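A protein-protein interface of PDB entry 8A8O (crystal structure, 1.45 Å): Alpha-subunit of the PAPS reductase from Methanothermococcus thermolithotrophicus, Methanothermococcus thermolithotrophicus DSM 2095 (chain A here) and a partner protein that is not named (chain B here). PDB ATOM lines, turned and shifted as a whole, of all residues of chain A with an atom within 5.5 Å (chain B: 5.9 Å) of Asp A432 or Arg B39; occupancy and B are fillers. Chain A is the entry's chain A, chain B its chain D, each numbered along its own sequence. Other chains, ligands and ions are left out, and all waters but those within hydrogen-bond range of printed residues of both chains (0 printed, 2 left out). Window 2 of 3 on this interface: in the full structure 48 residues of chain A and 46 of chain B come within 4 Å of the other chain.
Of the printed residues of chain B, Ala A201 touches Gln B61. Of chain B, only Arg B39 (3.9 Å) comes within 4 Å of Asp A432. Lys B38 touches none of the printed residues of chain A. Of the printed residues of chain A, Asp B40 touches Arg A202 and His A203. Printed residues of chain A within 4 Å of Cys B41: His A203. Printed residues of chain A within 4 Å of Gln B61: Ala A200 (3.0 Å) and Ala A201 (3.5 Å). The nearest printed residue of chain B that does not touch Gly A199 is Asp B40 (6.1 Å).
Among the printed residues, pairs that only touch across the chains: Arg A202 with Arg B39 (3.3 Å), Ala A201 with Gln B61 (3.5 Å), Ala A200 with Arg B39 (3.5 Å), Gly A199 with Arg B39 (3.6 Å), His A203 with Arg B39 (3.6 Å) and His A203 with Cys B41 (3.6 Å).
NH2 of Arg A202 is in salt-bridge range of OD2 of Asp A432, at 3.3 Å. OD1 of Asp A432 is in salt-bridge range of NZ of Lys A487 (2.8 Å). N of Thr B2 sits at hydrogen-bond distance from OE1 of Gln B61 (3.1 Å). The side-chain carboxylate (OD2) of Asp B37 lies within salt-bridge range of the guanidinium group (NH2) of Arg B39.
Of the 15 printed residues of chain A, 6 touch a printed residue of chain B. Printed residues of chain A that touch a printed residue of chain B: Gly A199, Ala A200, Ala A201, Arg A202, His A203 and Asp A432. Among the printed residues, Asp or Glu carboxylates within 4 Å of a Lys or Arg side-chain nitrogen of the other chain: Arg A202 with Asp B37 (3.5 Å), Arg A202 with Asp B40 (2.8 Å) and Asp A432 with Arg B39 (3.9 Å).
O of Ala A200 lies within hydrogen-bond range of NE2 of Gln B61 (3.0 Å). OD2 of Asp B37 is in salt-bridge range of NH2 of Arg A202, at 3.5 Å. The side-chain carboxylate of Asp B40 lies within salt-bridge range of the guanidinium group of Arg A202. The backbone carbonyl oxygen (O) of Asp B40 sits at hydrogen-bond distance from a ring nitrogen (ND1) of His A203, 2.8 Å away. The guanidinium group of Arg B39 is in salt-bridge range of the side-chain carboxylate of Asp A432.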
ATOM      1  N   GLY A 199     -21.235 -27.541 -14.707  1.00  0.00           N
ATOM      2  CA  GLY A 199     -20.884 -26.407 -15.565  1.00  0.00           C
ATOM      3  C   GLY A 199     -22.097 -25.520 -15.862  1.00  0.00           C
ATOM      4  O   GLY A 199     -22.653 -24.884 -14.953  1.00  0.00           O
ATOM      5  N   ALA A 200     -22.501 -25.491 -17.134  1.00  0.00           N
ATOM      6  CA  ALA A 200     -23.514 -24.542 -17.571  1.00  0.00           C
ATOM      7  C   ALA A 200     -24.819 -24.690 -16.803  1.00  0.00           C
ATOM      8  O   ALA A 200     -25.515 -23.695 -16.581  1.00  0.00           O
ATOM      9  CB  ALA A 200     -23.776 -24.717 -19.066  1.00  0.00           C
ATOM     10  N   ALA A 201     -25.167 -25.910 -16.400  1.00  0.00           N
ATOM     11  CA  ALA A 201     -26.438 -26.182 -15.731  1.00  0.00           C
ATOM     12  C   ALA A 201     -26.212 -26.792 -14.357  1.00  0.00           C
ATOM     13  O   ALA A 201     -26.988 -27.638 -13.887  1.00  0.00           O
ATOM     14  CB  ALA A 201     -27.308 -27.106 -16.581  1.00  0.00           C
ATOM     15  N   ARG A 202     -25.155 -26.340 -13.681  1.00  0.00           N
ATOM     16  CA  ARG A 202     -24.738 -26.964 -12.431  1.00  0.00           C
ATOM     17  C   ARG A 202     -25.771 -26.849 -11.313  1.00  0.00           C
ATOM     18  O   ARG A 202     -25.727 -27.663 -10.379  1.00  0.00           O
ATOM     19  CB  ARG A 202     -23.379 -26.417 -11.978  1.00  0.00           C
ATOM     20  CG  ARG A 202     -23.387 -24.952 -11.605  1.00  0.00           C
ATOM     21  CD  ARG A 202     -21.974 -24.371 -11.642  1.00  0.00           C
ATOM     22  NE  ARG A 202     -21.967 -23.002 -11.141  1.00  0.00           N
ATOM     23  CZ  ARG A 202     -20.915 -22.194 -11.174  1.00  0.00           C
ATOM     24  NH1 ARG A 202     -19.764 -22.577 -11.704  1.00  0.00           N
ATOM     25  NH2 ARG A 202     -21.024 -20.971 -10.664  1.00  0.00           N
ATOM     26  N   HIS A 203     -26.687 -25.879 -11.370  1.00  0.00           N
ATOM     27  CA  HIS A 203     -27.707 -25.753 -10.328  1.00  0.00           C
ATOM     28  C   HIS A 203     -29.068 -26.274 -10.767  1.00  0.00           C
ATOM     29  O   HIS A 203     -30.069 -26.013 -10.090  1.00  0.00           O
ATOM     30  CB  HIS A 203     -27.771 -24.306  -9.822  1.00  0.00           C
ATOM     31  CG  HIS A 203     -26.710 -24.006  -8.802  1.00  0.00           C
ATOM     32  ND1 HIS A 203     -26.678 -22.832  -8.090  1.00  0.00           N
ATOM     33  CD2 HIS A 203     -25.665 -24.746  -8.348  1.00  0.00           C
ATOM     34  CE1 HIS A 203     -25.653 -22.842  -7.257  1.00  0.00           C
ATOM     35  NE2 HIS A 203     -25.025 -23.995  -7.387  1.00  0.00           N
ATOM     36  N   SER A 430     -10.632 -19.232  -6.088  1.00  0.00           N
ATOM     37  CA  SER A 430     -11.988 -18.746  -5.914  1.00  0.00           C
ATOM     38  C   SER A 430     -12.868 -19.800  -5.259  1.00  0.00           C
ATOM     39  O   SER A 430     -12.569 -20.998  -5.289  1.00  0.00           O
ATOM     40  CB  SER A 430     -12.574 -18.367  -7.284  1.00  0.00           C
ATOM     41  OG  SER A 430     -12.872 -19.540  -8.027  1.00  0.00           O
ATOM     42  N   PRO A 431     -13.974 -19.391  -4.639  1.00  0.00           N
ATOM     43  CA  PRO A 431     -14.907 -20.402  -4.115  1.00  0.00           C
ATOM     44  C   PRO A 431     -15.401 -21.361  -5.185  1.00  0.00           C
ATOM     45  O   PRO A 431     -15.524 -22.558  -4.912  1.00  0.00           O
ATOM     46  CB  PRO A 431     -16.037 -19.556  -3.510  1.00  0.00           C
ATOM     47  CG  PRO A 431     -15.359 -18.233  -3.171  1.00  0.00           C
ATOM     48  CD  PRO A 431     -14.379 -18.013  -4.289  1.00  0.00           C
ATOM     49  N   ASP A 432     -15.674 -20.868  -6.398  1.00  0.00           N
ATOM     50  CA  ASP A 432     -16.176 -21.734  -7.466  1.00  0.00           C
ATOM     51  C   ASP A 432     -15.184 -22.841  -7.797  1.00  0.00           C
ATOM     52  O   ASP A 432     -15.573 -24.000  -7.977  1.00  0.00           O
ATOM     53  CB  ASP A 432     -16.467 -20.919  -8.725  1.00  0.00           C
ATOM     54  CG  ASP A 432     -17.821 -20.238  -8.688  1.00  0.00           C
ATOM     55  OD1 ASP A 432     -18.499 -20.305  -7.641  1.00  0.00           O
ATOM     56  OD2 ASP A 432     -18.207 -19.637  -9.715  1.00  0.00           O
ATOM     57  N   GLU A 433     -13.894 -22.501  -7.878  1.00  0.00           N
ATOM     58  CA  GLU A 433     -12.869 -23.500  -8.165  1.00  0.00           C
ATOM     59  C   GLU A 433     -12.829 -24.579  -7.090  1.00  0.00           C
ATOM     60  O   GLU A 433     -12.746 -25.778  -7.394  1.00  0.00           O
ATOM     61  CB  GLU A 433     -11.499 -22.813  -8.273  1.00  0.00           C
ATOM     62  CG  GLU A 433     -11.321 -22.006  -9.541  1.00  0.00           C
ATOM     63  CD  GLU A 433     -10.039 -21.183  -9.556  1.00  0.00           C
ATOM     64  OE1 GLU A 433      -9.587 -20.719  -8.485  1.00  0.00           O
ATOM     65  OE2 GLU A 433      -9.485 -20.999 -10.659  1.00  0.00           O
ATOM     66  N   ILE A 434     -12.849 -24.173  -5.821  1.00  0.00           N
ATOM     67  CA  ILE A 434     -12.758 -25.146  -4.742  1.00  0.00           C
ATOM     68  C   ILE A 434     -14.038 -25.975  -4.675  1.00  0.00           C
ATOM     69  O   ILE A 434     -14.000 -27.171  -4.378  1.00  0.00           O
ATOM     70  CB  ILE A 434     -12.462 -24.431  -3.413  1.00  0.00           C
ATOM     71  CG1 ILE A 434     -11.108 -23.708  -3.446  1.00  0.00           C
ATOM     72  CG2 ILE A 434     -12.484 -25.419  -2.259  1.00  0.00           C
ATOM     73  CD1 ILE A 434      -9.947 -24.535  -3.975  1.00  0.00           C
ATOM     74  N   GLU A 435     -15.186 -25.355  -4.956  1.00  0.00           N
ATOM     75  CA  GLU A 435     -16.445 -26.095  -4.968  1.00  0.00           C
ATOM     76  C   GLU A 435     -16.394 -27.224  -5.993  1.00  0.00           C
ATOM     77  O   GLU A 435     -16.778 -28.365  -5.690  1.00  0.00           O
ATOM     78  CB  GLU A 435     -17.597 -25.145  -5.270  1.00  0.00           C
ATOM     79  CG  GLU A 435     -18.958 -25.794  -5.310  1.00  0.00           C
ATOM     80  CD  GLU A 435     -20.016 -24.921  -5.968  1.00  0.00           C
ATOM     81  OE1 GLU A 435     -19.733 -23.782  -6.407  1.00  0.00           O
ATOM     82  OE2 GLU A 435     -21.180 -25.319  -5.886  1.00  0.00           O
ATOM     83  N   GLU A 436     -15.888 -26.932  -7.193  1.00  0.00           N
ATOM     84  CA  GLU A 436     -15.801 -27.956  -8.229  1.00  0.00           C
ATOM     85  C   GLU A 436     -14.827 -29.047  -7.827  1.00  0.00           C
ATOM     86  O   GLU A 436     -15.075 -30.237  -8.062  1.00  0.00           O
ATOM     87  CB  GLU A 436     -15.396 -27.336  -9.559  1.00  0.00           C
ATOM     88  CG  GLU A 436     -16.474 -26.425 -10.158  1.00  0.00           C
ATOM     89  CD  GLU A 436     -16.109 -25.874 -11.527  1.00  0.00           C
ATOM     90  OE1 GLU A 436     -15.592 -26.648 -12.359  1.00  0.00           O
ATOM     91  OE2 GLU A 436     -16.339 -24.665 -11.768  1.00  0.00           O
ATOM     92  N   ARG A 437     -13.719 -28.664  -7.198  1.00  0.00           N
ATOM     93  CA  ARG A 437     -12.743 -29.639  -6.723  1.00  0.00           C
ATOM     94  C   ARG A 437     -13.366 -30.595  -5.714  1.00  0.00           C
ATOM     95  O   ARG A 437     -13.176 -31.816  -5.797  1.00  0.00           O
ATOM     96  CB  ARG A 437     -11.582 -28.883  -6.087  1.00  0.00           C
ATOM     97  CG  ARG A 437     -10.425 -29.744  -5.636  1.00  0.00           C
ATOM     98  CD  ARG A 437      -9.265 -28.862  -5.209  1.00  0.00           C
ATOM     99  NE  ARG A 437      -8.405 -29.537  -4.248  1.00  0.00           N
ATOM    100  CZ  ARG A 437      -7.548 -28.922  -3.445  1.00  0.00           C
ATOM    101  NH1 ARG A 437      -7.366 -27.616  -3.502  1.00  0.00           N
ATOM    102  NH2 ARG A 437      -6.868 -29.635  -2.558  1.00  0.00           N
ATOM    103  N   LYS A 487     -20.585 -17.285  -0.962  1.00  0.00           N
ATOM    104  CA  LYS A 487     -20.220 -18.517  -1.659  1.00  0.00           C
ATOM    105  C   LYS A 487     -19.040 -19.207  -0.977  1.00  0.00           C
ATOM    106  O   LYS A 487     -18.984 -20.442  -0.904  1.00  0.00           O
ATOM    107  CB  LYS A 487     -19.892 -18.209  -3.123  1.00  0.00           C
ATOM    108  CG  LYS A 487     -21.124 -17.882  -3.975  1.00  0.00           C
ATOM    109  CD  LYS A 487     -20.810 -17.632  -5.460  1.00  0.00           C
ATOM    110  CE  LYS A 487     -19.386 -17.994  -5.862  1.00  0.00           C
ATOM    111  NZ  LYS A 487     -19.104 -17.619  -7.282  1.00  0.00           N
ATOM    112  N   VAL A 491     -18.967 -23.104   0.671  1.00  0.00           N
ATOM    113  CA  VAL A 491     -17.934 -24.117   0.445  1.00  0.00           C
ATOM    114  C   VAL A 491     -17.354 -24.601   1.767  1.00  0.00           C
ATOM    115  O   VAL A 491     -17.174 -25.808   1.977  1.00  0.00           O
ATOM    116  CB  VAL A 491     -16.838 -23.571  -0.484  1.00  0.00           C
ATOM    117  CG1 VAL A 491     -15.698 -24.575  -0.636  1.00  0.00           C
ATOM    118  CG2 VAL A 491     -17.416 -23.224  -1.861  1.00  0.00           C
ATOM    119  N   THR B   2     -32.088 -21.631 -17.325  1.00  0.00           N
ATOM    120  CA  THR B   2     -31.582 -20.395 -16.689  1.00  0.00           C
ATOM    121  C   THR B   2     -32.413 -19.216 -17.190  1.00  0.00           C
ATOM    122  O   THR B   2     -33.436 -19.405 -17.886  1.00  0.00           O
ATOM    123  CB  THR B   2     -30.081 -20.199 -16.974  1.00  0.00           C
ATOM    124  OG1 THR B   2     -29.593 -19.087 -16.203  1.00  0.00           O
ATOM    125  CG2 THR B   2     -29.816 -19.975 -18.459  1.00  0.00           C
ATOM    126  N   ASP B  37     -24.452 -14.929 -12.013  1.00  0.00           N
ATOM    127  CA  ASP B  37     -23.921 -16.035 -12.803  1.00  0.00           C
ATOM    128  C   ASP B  37     -25.097 -16.881 -13.260  1.00  0.00           C
ATOM    129  O   ASP B  37     -25.769 -17.522 -12.435  1.00  0.00           O
ATOM    130  CB  ASP B  37     -22.952 -16.894 -11.995  1.00  0.00           C
ATOM    131  CG  ASP B  37     -22.070 -17.747 -12.880  1.00  0.00           C
ATOM    132  OD1 ASP B  37     -22.559 -18.218 -13.936  1.00  0.00           O
ATOM    133  OD2 ASP B  37     -20.888 -17.948 -12.517  1.00  0.00           O
ATOM    134  N   LYS B  38     -25.337 -16.900 -14.574  1.00  0.00           N
ATOM    135  CA  LYS B  38     -26.471 -17.653 -15.095  1.00  0.00           C
ATOM    136  C   LYS B  38     -26.344 -19.142 -14.824  1.00  0.00           C
ATOM    137  O   LYS B  38     -27.367 -19.844 -14.823  1.00  0.00           O
ATOM    138  CB  LYS B  38     -26.611 -17.397 -16.601  1.00  0.00           C
ATOM    139  CG  LYS B  38     -25.550 -18.075 -17.440  1.00  0.00           C
ATOM    140  CD  LYS B  38     -25.695 -17.759 -18.925  1.00  0.00           C
ATOM    141  CE  LYS B  38     -24.419 -18.092 -19.680  1.00  0.00           C
ATOM    142  NZ  LYS B  38     -24.520 -17.791 -21.136  1.00  0.00           N
ATOM    143  N   ARG B  39     -25.123 -19.644 -14.607  1.00  0.00           N
ATOM    144  CA  ARG B  39     -24.951 -21.071 -14.322  1.00  0.00           C
ATOM    145  C   ARG B  39     -25.539 -21.479 -12.975  1.00  0.00           C
ATOM    146  O   ARG B  39     -25.778 -22.677 -12.754  1.00  0.00           O
ATOM    147  CB  ARG B  39     -23.474 -21.443 -14.347  1.00  0.00           C
ATOM    148  CG  ARG B  39     -22.846 -21.276 -15.703  1.00  0.00           C
ATOM    149  CD  ARG B  39     -21.349 -21.504 -15.632  1.00  0.00           C
ATOM    150  NE  ARG B  39     -20.690 -20.566 -14.730  1.00  0.00           N
ATOM    151  CZ  ARG B  39     -19.408 -20.620 -14.391  1.00  0.00           C
ATOM    152  NH1 ARG B  39     -18.605 -21.566 -14.860  1.00  0.00           N
ATOM    153  NH2 ARG B  39     -18.919 -19.701 -13.567  1.00  0.00           N
ATOM    154  N   ASP B  40     -25.768 -20.528 -12.069  1.00  0.00           N
ATOM    155  CA  ASP B  40     -26.251 -20.839 -10.728  1.00  0.00           C
ATOM    156  C   ASP B  40     -27.768 -20.788 -10.611  1.00  0.00           C
ATOM    157  O   ASP B  40     -28.291 -21.018  -9.520  1.00  0.00           O
ATOM    158  CB  ASP B  40     -25.590 -19.919  -9.707  1.00  0.00           C
ATOM    159  CG  ASP B  40     -24.119 -20.252  -9.500  1.00  0.00           C
ATOM    160  OD1 ASP B  40     -23.747 -21.436  -9.679  1.00  0.00           O
ATOM    161  OD2 ASP B  40     -23.341 -19.341  -9.151  1.00  0.00           O
ATOM    162  N   CYS B  41     -28.477 -20.506 -11.703  1.00  0.00           N
ATOM    163  CA  CYS B  41     -29.931 -20.469 -11.696  1.00  0.00           C
ATOM    164  C   CYS B  41     -30.531 -21.868 -11.562  1.00  0.00           C
ATOM    165  O   CYS B  41     -30.083 -22.830 -12.205  1.00  0.00           O
ATOM    166  CB  CYS B  41     -30.448 -19.775 -12.962  1.00  0.00           C
ATOM    167  SG  CYS B  41     -32.231 -19.639 -13.087  1.00  0.00           S
ATOM    168  N   GLN B  61     -30.356 -24.069 -20.985  1.00  0.00           N
ATOM    169  CA  GLN B  61     -28.974 -23.911 -21.408  1.00  0.00           C
ATOM    170  C   GLN B  61     -28.726 -24.705 -22.688  1.00  0.00           C
ATOM    171  O   GLN B  61     -29.023 -25.909 -22.736  1.00  0.00           O
ATOM    172  CB  GLN B  61     -28.055 -24.431 -20.296  1.00  0.00           C
ATOM    173  CG  GLN B  61     -27.908 -23.480 -19.095  1.00  0.00           C
ATOM    174  CD  GLN B  61     -28.975 -23.666 -18.002  1.00  0.00           C
ATOM    175  OE1 GLN B  61     -30.166 -23.833 -18.276  1.00  0.00           O
ATOM    176  NE2 GLN B  61     -28.550 -23.583 -16.758  1.00  0.00           N
